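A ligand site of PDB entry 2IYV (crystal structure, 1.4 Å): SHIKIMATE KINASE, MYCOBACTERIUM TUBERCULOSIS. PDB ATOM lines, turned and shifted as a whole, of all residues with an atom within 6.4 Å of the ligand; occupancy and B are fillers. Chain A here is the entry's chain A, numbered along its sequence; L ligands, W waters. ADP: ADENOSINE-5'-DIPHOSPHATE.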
ATOM      1  N   GLY A   9      21.877 -17.812  -2.388  1.00  0.00           N
ATOM      2  CA  GLY A   9      21.330 -17.781  -1.037  1.00  0.00           C
ATOM      3  C   GLY A   9      20.692 -16.465  -0.726  1.00  0.00           C
ATOM      4  O   GLY A   9      20.820 -15.480  -1.468  1.00  0.00           O
ATOM      5  N   LEU A  10      20.044 -16.446   0.446  1.00  0.00           N
ATOM      6  CA  LEU A  10      19.307 -15.296   0.939  1.00  0.00           C
ATOM      7  C   LEU A  10      20.257 -14.180   1.379  1.00  0.00           C
ATOM      8  O   LEU A  10      21.468 -14.394   1.496  1.00  0.00           O
ATOM      9  CB  LEU A  10      18.456 -15.721   2.135  1.00  0.00           C
ATOM     10  CG  LEU A  10      17.313 -16.668   1.849  1.00  0.00           C
ATOM     11  CD1 LEU A  10      16.765 -17.254   3.133  1.00  0.00           C
ATOM     12  CD2 LEU A  10      16.248 -15.934   1.007  1.00  0.00           C
ATOM     13  N   PRO A  11      19.717 -12.975   1.601  1.00  0.00           N
ATOM     14  CA  PRO A  11      20.555 -11.898   2.106  1.00  0.00           C
ATOM     15  C   PRO A  11      21.177 -12.279   3.442  1.00  0.00           C
ATOM     16  O   PRO A  11      20.516 -12.831   4.307  1.00  0.00           O
ATOM     17  CB  PRO A  11      19.575 -10.730   2.231  1.00  0.00           C
ATOM     18  CG  PRO A  11      18.462 -11.059   1.288  1.00  0.00           C
ATOM     19  CD  PRO A  11      18.324 -12.525   1.430  1.00  0.00           C
ATOM     20  N   GLY A  12      22.465 -12.044   3.573  1.00  0.00           N
ATOM     21  CA  GLY A  12      23.155 -12.406   4.802  1.00  0.00           C
ATOM     22  C   GLY A  12      23.700 -13.821   4.838  1.00  0.00           C
ATOM     23  O   GLY A  12      24.435 -14.182   5.748  1.00  0.00           O
ATOM     24  N   SER A  13      23.396 -14.628   3.844  1.00  0.00           N
ATOM     25  CA  SER A  13      23.852 -16.007   3.828  1.00  0.00           C
ATOM     26  C   SER A  13      25.357 -16.139   3.648  1.00  0.00           C
ATOM     27  O   SER A  13      25.944 -17.159   4.036  1.00  0.00           O
ATOM     28  CB  SER A  13      23.130 -16.828   2.767  1.00  0.00           C
ATOM     29  OG  SER A  13      23.306 -16.362   1.443  1.00  0.00           O
ATOM     30  N   GLY A  14      25.980 -15.099   3.117  1.00  0.00           N
ATOM     31  CA  GLY A  14      27.413 -15.043   2.969  1.00  0.00           C
ATOM     32  C   GLY A  14      27.924 -14.967   1.550  1.00  0.00           C
ATOM     33  O   GLY A  14      29.074 -15.292   1.290  1.00  0.00           O
ATOM     34  N   LYS A  15      27.078 -14.602   0.590  1.00  0.00           N
ATOM     35  CA  LYS A  15      27.532 -14.533  -0.813  1.00  0.00           C
ATOM     36  C   LYS A  15      28.777 -13.647  -1.006  1.00  0.00           C
ATOM     37  O   LYS A  15      29.737 -14.034  -1.701  1.00  0.00           O
ATOM     38  CB  LYS A  15      26.397 -14.110  -1.725  1.00  0.00           C
ATOM     39  CG  LYS A  15      25.248 -15.151  -1.788  1.00  0.00           C
ATOM     40  CD  LYS A  15      24.132 -14.704  -2.712  1.00  0.00           C
ATOM     41  CE  LYS A  15      23.442 -13.420  -2.301  1.00  0.00           C
ATOM     42  NZ  LYS A  15      22.878 -13.425  -0.927  1.00  0.00           N
ATOM     43  N   SER A  16      28.770 -12.480  -0.387  1.00  0.00           N
ATOM     44  CA  SER A  16      29.906 -11.586  -0.490  1.00  0.00           C
ATOM     45  C   SER A  16      31.122 -12.136   0.294  1.00  0.00           C
ATOM     46  O   SER A  16      32.239 -12.181  -0.204  1.00  0.00           O
ATOM     47  CB  SER A  16      29.535 -10.202   0.050  1.00  0.00           C
ATOM     48  OG  SER A  16      28.377  -9.684  -0.563  1.00  0.00           O
ATOM     49  N   THR A  17      30.886 -12.515   1.541  1.00  0.00           N
ATOM     50  CA  THR A  17      31.946 -12.960   2.440  1.00  0.00           C
ATOM     51  C   THR A  17      32.572 -14.274   1.996  1.00  0.00           C
ATOM     52  O   THR A  17      33.801 -14.427   1.895  1.00  0.00           O
ATOM     53  CB  THR A  17      31.356 -13.154   3.835  1.00  0.00           C
ATOM     54  OG1 THR A  17      30.800 -11.924   4.325  1.00  0.00           O
ATOM     55  CG2 THR A  17      32.418 -13.645   4.820  1.00  0.00           C
ATOM     56  N   ILE A  18      31.718 -15.229   1.718  1.00  0.00           N
ATOM     57  CA  ILE A  18      32.193 -16.514   1.196  1.00  0.00           C
ATOM     58  C   ILE A  18      32.737 -16.376  -0.236  1.00  0.00           C
ATOM     59  O   ILE A  18      33.728 -16.997  -0.557  1.00  0.00           O
ATOM     60  CB  ILE A  18      31.094 -17.598   1.244  1.00  0.00           C
ATOM     61  CG1 ILE A  18      30.567 -17.760   2.691  1.00  0.00           C
ATOM     62  CG2 ILE A  18      31.600 -18.951   0.764  1.00  0.00           C
ATOM     63  CD1 ILE A  18      31.594 -18.002   3.745  1.00  0.00           C
ATOM     64  N   ARG A  20      34.371 -13.859  -1.488  1.00  0.00           N
ATOM     65  CA  ARG A  20      35.717 -13.335  -1.376  1.00  0.00           C
ATOM     66  C   ARG A  20      36.671 -14.385  -0.809  1.00  0.00           C
ATOM     67  O   ARG A  20      37.775 -14.569  -1.303  1.00  0.00           O
ATOM     68  CB  ARG A  20      35.732 -12.072  -0.503  1.00  0.00           C
ATOM     69  CG  ARG A  20      35.143 -10.844  -1.178  1.00  0.00           C
ATOM     70  CD  ARG A  20      35.318  -9.563  -0.364  1.00  0.00           C
ATOM     71  NE  ARG A  20      34.522  -9.583   0.860  1.00  0.00           N
ATOM     72  CZ  ARG A  20      34.971  -9.947   2.056  1.00  0.00           C
ATOM     73  NH1 ARG A  20      36.231 -10.340   2.229  1.00  0.00           N
ATOM     74  NH2 ARG A  20      34.143  -9.918   3.099  1.00  0.00           N
ATOM     75  N   LEU A 100      24.161 -21.473   0.016  1.00  0.00           N
ATOM     76  CA  LEU A 100      24.528 -21.083   1.379  1.00  0.00           C
ATOM     77  C   LEU A 100      23.224 -20.940   2.142  1.00  0.00           C
ATOM     78  O   LEU A 100      22.454 -20.002   1.909  1.00  0.00           O
ATOM     79  CB  LEU A 100      25.234 -19.734   1.324  1.00  0.00           C
ATOM     80  CG  LEU A 100      26.529 -19.689   0.517  1.00  0.00           C
ATOM     81  CD1 LEU A 100      27.057 -18.285   0.500  1.00  0.00           C
ATOM     82  CD2 LEU A 100      27.552 -20.668   1.041  1.00  0.00           C
ATOM     83  N   GLU A 106      18.715 -15.786  11.662  1.00  0.00           N
ATOM     84  CA  GLU A 106      20.127 -15.487  11.412  1.00  0.00           C
ATOM     85  C   GLU A 106      20.321 -14.534  10.235  1.00  0.00           C
ATOM     86  O   GLU A 106      21.178 -13.694  10.244  1.00  0.00           O
ATOM     87  CB  GLU A 106      20.891 -16.787  11.222  1.00  0.00           C
ATOM     88  CG  GLU A 106      22.374 -16.660  11.000  1.00  0.00           C
ATOM     89  CD  GLU A 106      23.170 -16.189  12.210  1.00  0.00           C
ATOM     90  OE1 GLU A 106      22.592 -15.929  13.309  1.00  0.00           O
ATOM     91  OE2 GLU A 106      24.418 -16.101  12.052  1.00  0.00           O
ATOM     92  N   ARG A 109      19.464 -11.100  11.457  1.00  0.00           N
ATOM     93  CA  ARG A 109      20.582 -10.597  12.289  1.00  0.00           C
ATOM     94  C   ARG A 109      21.764 -10.144  11.433  1.00  0.00           C
ATOM     95  O   ARG A 109      22.309  -9.072  11.619  1.00  0.00           O
ATOM     96  CB  ARG A 109      21.048 -11.686  13.240  1.00  0.00           C
ATOM     97  CG  ARG A 109      22.139 -11.231  14.176  1.00  0.00           C
ATOM     98  CD  ARG A 109      22.713 -12.354  14.999  1.00  0.00           C
ATOM     99  NE  ARG A 109      23.579 -13.257  14.195  1.00  0.00           N
ATOM    100  CZ  ARG A 109      24.818 -12.979  13.790  1.00  0.00           C
ATOM    101  NH1 ARG A 109      25.374 -11.827  14.018  1.00  0.00           N
ATOM    102  NH2 ARG A 109      25.548 -13.884  13.186  1.00  0.00           N
ATOM    103  N   ARG A 110      22.140 -10.977  10.465  1.00  0.00           N
ATOM    104  CA  ARG A 110      23.304 -10.718   9.641  1.00  0.00           C
ATOM    105  C   ARG A 110      23.111  -9.593   8.620  1.00  0.00           C
ATOM    106  O   ARG A 110      24.078  -9.148   7.968  1.00  0.00           O
ATOM    107  CB  ARG A 110      23.687 -11.963   8.884  1.00  0.00           C
ATOM    108  CG  ARG A 110      24.329 -13.013   9.684  1.00  0.00           C
ATOM    109  CD  ARG A 110      24.908 -14.015   8.714  1.00  0.00           C
ATOM    110  NE  ARG A 110      25.206 -15.258   9.364  1.00  0.00           N
ATOM    111  CZ  ARG A 110      25.454 -16.400   8.744  1.00  0.00           C
ATOM    112  NH1 ARG A 110      25.701 -17.468   9.470  1.00  0.00           N
ATOM    113  NH2 ARG A 110      25.441 -16.487   7.408  1.00  0.00           N
ATOM    114  N   THR A 111      21.890  -9.116   8.481  1.00  0.00           N
ATOM    115  CA  THR A 111      21.596  -7.998   7.583  1.00  0.00           C
ATOM    116  C   THR A 111      21.120  -6.750   8.321  1.00  0.00           C
ATOM    117  O   THR A 111      20.513  -5.860   7.735  1.00  0.00           O
ATOM    118  CB  THR A 111      20.609  -8.412   6.500  1.00  0.00           C
ATOM    119  OG1 THR A 111      19.382  -8.899   7.052  1.00  0.00           O
ATOM    120  CG2 THR A 111      21.190  -9.520   5.654  1.00  0.00           C
ATOM    121  N   THR A 150      25.111 -22.449   6.954  1.00  0.00           N
ATOM    122  CA  THR A 150      26.005 -21.410   7.479  1.00  0.00           C
ATOM    123  C   THR A 150      25.578 -20.888   8.834  1.00  0.00           C
ATOM    124  O   THR A 150      26.202 -19.989   9.351  1.00  0.00           O
ATOM    125  CB  THR A 150      26.113 -20.188   6.535  1.00  0.00           C
ATOM    126  OG1 THR A 150      24.911 -19.406   6.594  1.00  0.00           O
ATOM    127  CG2 THR A 150      26.414 -20.577   5.092  1.00  0.00           C
ATOM    128  N   ASN A 151      24.494 -21.414   9.404  1.00  0.00           N
ATOM    129  CA  ASN A 151      24.019 -20.921  10.707  1.00  0.00           C
ATOM    130  C   ASN A 151      25.032 -21.112  11.834  1.00  0.00           C
ATOM    131  O   ASN A 151      25.145 -20.237  12.711  1.00  0.00           O
ATOM    132  CB  ASN A 151      22.711 -21.605  11.083  1.00  0.00           C
ATOM    133  CG  ASN A 151      21.574 -21.216  10.184  1.00  0.00           C
ATOM    134  OD1 ASN A 151      21.259 -20.042  10.056  1.00  0.00           O
ATOM    135  ND2 ASN A 151      20.977 -22.202   9.518  1.00  0.00           N
ATOM    136  N   ARG A 153      28.406 -22.469  11.223  1.00  0.00           N
ATOM    137  CA  ARG A 153      29.775 -22.484  10.734  1.00  0.00           C
ATOM    138  C   ARG A 153      30.223 -21.071  10.516  1.00  0.00           C
ATOM    139  O   ARG A 153      29.531 -20.311   9.826  1.00  0.00           O
ATOM    140  CB  ARG A 153      29.877 -23.216   9.415  1.00  0.00           C
ATOM    141  CG  ARG A 153      29.609 -24.680   9.463  1.00  0.00           C
ATOM    142  CD  ARG A 153      29.891 -25.283   8.115  1.00  0.00           C
ATOM    143  NE  ARG A 153      29.792 -26.736   8.086  1.00  0.00           N
ATOM    144  CZ  ARG A 153      28.672 -27.412   7.912  1.00  0.00           C
ATOM    145  NH1 ARG A 153      27.520 -26.787   7.762  1.00  0.00           N
ATOM    146  NH2 ARG A 153      28.693 -28.740   7.910  1.00  0.00           N
ATOM    147  N   ASN A 154      31.405 -20.715  11.028  1.00  0.00           N
ATOM    148  CA  ASN A 154      32.014 -19.425  10.657  1.00  0.00           C
ATOM    149  C   ASN A 154      32.499 -19.430   9.206  1.00  0.00           C
ATOM    150  O   ASN A 154      32.508 -20.477   8.562  1.00  0.00           O
ATOM    151  CB  ASN A 154      33.122 -19.004  11.649  1.00  0.00           C
ATOM    152  CG  ASN A 154      34.273 -19.952  11.706  1.00  0.00           C
ATOM    153  OD1 ASN A 154      34.731 -20.464  10.707  1.00  0.00           O
ATOM    154  ND2 ASN A 154      34.782 -20.174  12.912  1.00  0.00           N
ATOM    155  N   PRO A 155      32.802 -18.250   8.669  1.00  0.00           N
ATOM    156  CA  PRO A 155      33.185 -18.218   7.244  1.00  0.00           C
ATOM    157  C   PRO A 155      34.317 -19.163   6.863  1.00  0.00           C
ATOM    158  O   PRO A 155      34.279 -19.782   5.801  1.00  0.00           O
ATOM    159  CB  PRO A 155      33.519 -16.762   7.000  1.00  0.00           C
ATOM    160  CG  PRO A 155      32.636 -16.035   7.975  1.00  0.00           C
ATOM    161  CD  PRO A 155      32.664 -16.884   9.211  1.00  0.00           C
ATOM    162  N   GLY A 156      35.351 -19.265   7.658  1.00  0.00           N
ATOM    163  CA  GLY A 156      36.436 -20.183   7.372  1.00  0.00           C
ATOM    164  C   GLY A 156      35.988 -21.637   7.291  1.00  0.00           C
ATOM    165  O   GLY A 156      36.446 -22.413   6.434  1.00  0.00           O
ATOM    166  N   VAL A 158      32.878 -22.612   6.585  1.00  0.00           N
ATOM    167  CA  VAL A 158      32.089 -22.707   5.361  1.00  0.00           C
ATOM    168  C   VAL A 158      32.993 -22.934   4.146  1.00  0.00           C
ATOM    169  O   VAL A 158      32.721 -23.830   3.318  1.00  0.00           O
ATOM    170  CB  VAL A 158      31.231 -21.459   5.174  1.00  0.00           C
ATOM    171  CG1 VAL A 158      30.544 -21.500   3.791  1.00  0.00           C
ATOM    172  CG2 VAL A 158      30.176 -21.340   6.256  1.00  0.00           C
HETATM  173  PB  ADP L   1      25.268 -11.654   1.438  1.00  0.00           P
HETATM  174  O1B ADP L   1      24.792 -13.085   1.190  1.00  0.00           O
HETATM  175  O2B ADP L   1      24.120 -10.693   1.694  1.00  0.00           O
HETATM  176  O3B ADP L   1      26.333 -11.148   0.475  1.00  0.00           O
HETATM  177  PA  ADP L   1      27.370 -11.100   3.406  1.00  0.00           P
HETATM  178  O1A ADP L   1      27.381  -9.639   3.122  1.00  0.00           O
HETATM  179  O2A ADP L   1      28.529 -11.933   2.964  1.00  0.00           O
HETATM  180  O3A ADP L   1      25.973 -11.745   2.889  1.00  0.00           O
HETATM  181  O5' ADP L   1      27.324 -11.351   4.989  1.00  0.00           O
HETATM  182  C5' ADP L   1      26.480 -10.526   5.784  1.00  0.00           C
HETATM  183  C4' ADP L   1      27.050 -10.400   7.187  1.00  0.00           C
HETATM  184  O4' ADP L   1      27.074 -11.698   7.778  1.00  0.00           O
HETATM  185  C3' ADP L   1      28.466  -9.881   7.225  1.00  0.00           C
HETATM  186  O3' ADP L   1      28.622  -9.082   8.398  1.00  0.00           O
HETATM  187  C2' ADP L   1      29.303 -11.117   7.368  1.00  0.00           C
HETATM  188  O2' ADP L   1      30.532 -10.932   8.055  1.00  0.00           O
HETATM  189  C1' ADP L   1      28.405 -12.045   8.154  1.00  0.00           C
HETATM  190  N9  ADP L   1      28.592 -13.457   7.854  1.00  0.00           N
HETATM  191  C8  ADP L   1      28.571 -14.014   6.593  1.00  0.00           C
HETATM  192  N7  ADP L   1      28.732 -15.339   6.644  1.00  0.00           N
HETATM  193  C5  ADP L   1      28.848 -15.632   7.984  1.00  0.00           C
HETATM  194  C6  ADP L   1      29.031 -16.848   8.772  1.00  0.00           C
HETATM  195  N6  ADP L   1      29.125 -18.005   8.119  1.00  0.00           N
HETATM  196  N1  ADP L   1      29.072 -16.778  10.153  1.00  0.00           N
HETATM  197  C2  ADP L   1      28.962 -15.588  10.750  1.00  0.00           C
HETATM  198  N3  ADP L   1      28.784 -14.428  10.130  1.00  0.00           N
HETATM  199  C4  ADP L   1      28.725 -14.399   8.756  1.00  0.00           C
HETATM  200  O   HOH W   1      30.062  -8.529   3.439  1.00  0.00           O
HETATM  201  O   HOH W   2      32.079  -9.980   5.769  1.00  0.00           O
HETATM  202  O   HOH W   3      23.844  -8.442   3.181  1.00  0.00           O
HETATM  203  O   HOH W   4      26.573  -7.771   1.188  1.00  0.00           O
HETATM  204  O   HOH W   5      26.041 -10.223  -1.907  1.00  0.00           O
HETATM  205  O   HOH W   6      28.161 -12.429  11.959  1.00  0.00           O
HETATM  206  O   HOH W   7      22.563 -10.183  -0.472  1.00  0.00           O
HETATM  207  O   HOH W   8      26.978 -10.314  11.043  1.00  0.00           O
HETATM  208  O   HOH W   9      27.591 -18.849  11.679  1.00  0.00           O
HETATM  209  O   HOH W  10      28.353 -17.747   5.247  1.00  0.00           O
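The guanidinium group (NH1) of Arg 110 lies within hydrogen-bond range of the backbone carbonyl oxygen (O) of Thr 150 (2.6 Å). The side-chain amide oxygen (OD1) of Asn 154 lies close to the backbone NH (N) of Gly 156 (3.3 Å). O of Gly 12 lies close to NH2 of Arg 110 (3.0 Å). The side-chain carboxylate of Glu 106 is in salt-bridge range of the guanidinium group of Arg 110 (2.9 Å). OG of Ser 13 sits at hydrogen-bond distance from O of Leu 10 (2.7 Å). NZ of Lys 15 lies within hydrogen-bond range of O of Gly 9, at 3.0 Å. The guanidinium group of Arg 110 sits at hydrogen-bond distance from the backbone carbonyl oxygen of Ser 13 (3.5 Å). NZ of Lys 15 sits at hydrogen-bond distance from O of Leu 10.
Water W5 bridges an oxygen (O3B) of the ligand and the side-chain hydroxyl (OG) of Ser 16. Water W7 lies within hydrogen-bond range of an oxygen (O2B) of the ligand and the side-chain amino group of Lys 15. Water W6 lies within hydrogen-bond range of a nitrogen (N3) of the ligand (2.8 Å) and the guanidinium group (NH2) of Arg 109 (3.2 Å). Water W4 bridges an oxygen (O1A) of the ligand (2.8 Å) and the side-chain hydroxyl of Ser 16 (3.2 Å). Water W10 bridges O of Ser 13 (2.8 Å) and N7 of the ligand (2.8 Å). Water W2 lies within hydrogen-bond range of OG1 of Thr 17 (2.7 Å), O2' of the ligand (2.9 Å) and NH2 of Arg 20 (3.4 Å).
Leu 10 touches the ligand. Pro 11 touches the ligand (C to O2B, 3.8 Å). Arg 110 touches the ligand (CD to O4', 3.3 Å). O of Thr 150 touches N6 of the ligand, at 3.7 Å. Asn 154 touches the ligand (C to N6, 3.8 Å). CD of Pro 155 touches C6 of the ligand, 3.7 Å away. Val 158 touches the ligand (CG2 to N6, 3.96 Å). Hydrophobic or aromatic side chains within 4 Å of the ligand: Pro 155 and Val 158. Within 4 Å of the ligand: Leu 10, Pro 11, Gly 12, Ser 13, Gly 14, Lys 15, Ser 16, Thr 17, Arg 110, Thr 150, Arg 153, Asn 154, Pro 155 and Val 158. Along chain A the residues within 4 Å of the ligand span positions 10 to 158.
O2A of the ligand sits at hydrogen-bond distance from N of Thr 17. An oxygen (O1B) of the ligand sits at hydrogen-bond distance from the backbone NH (N) of Ser 13 (3.4 Å). An oxygen (O3B) of the ligand is in hydrogen-bond range of the backbone NH (N) of Ser 16, 2.9 Å away. An oxygen (O1B) of the ligand is in salt-bridge range of the side-chain amino group of Lys 15 (2.9 Å). An oxygen (O1B) of the ligand lies within hydrogen-bond range of the backbone NH (N) of Lys 15 (2.8 Å). O of Arg 153 is in hydrogen-bond range of N6 of the ligand (2.9 Å). O3B of the ligand lies within hydrogen-bond range of OG of Ser 16 (2.7 Å). The side-chain hydroxyl of Thr 17 lies within hydrogen-bond range of an oxygen (O2A) of the ligand (2.6 Å). The backbone NH (N) of Gly 12 sits at hydrogen-bond distance from an oxygen (O2B) of the ligand. The backbone NH (N) of Gly 14 lies within hydrogen-bond range of an oxygen (O1B) of the ligand (3.0 Å).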
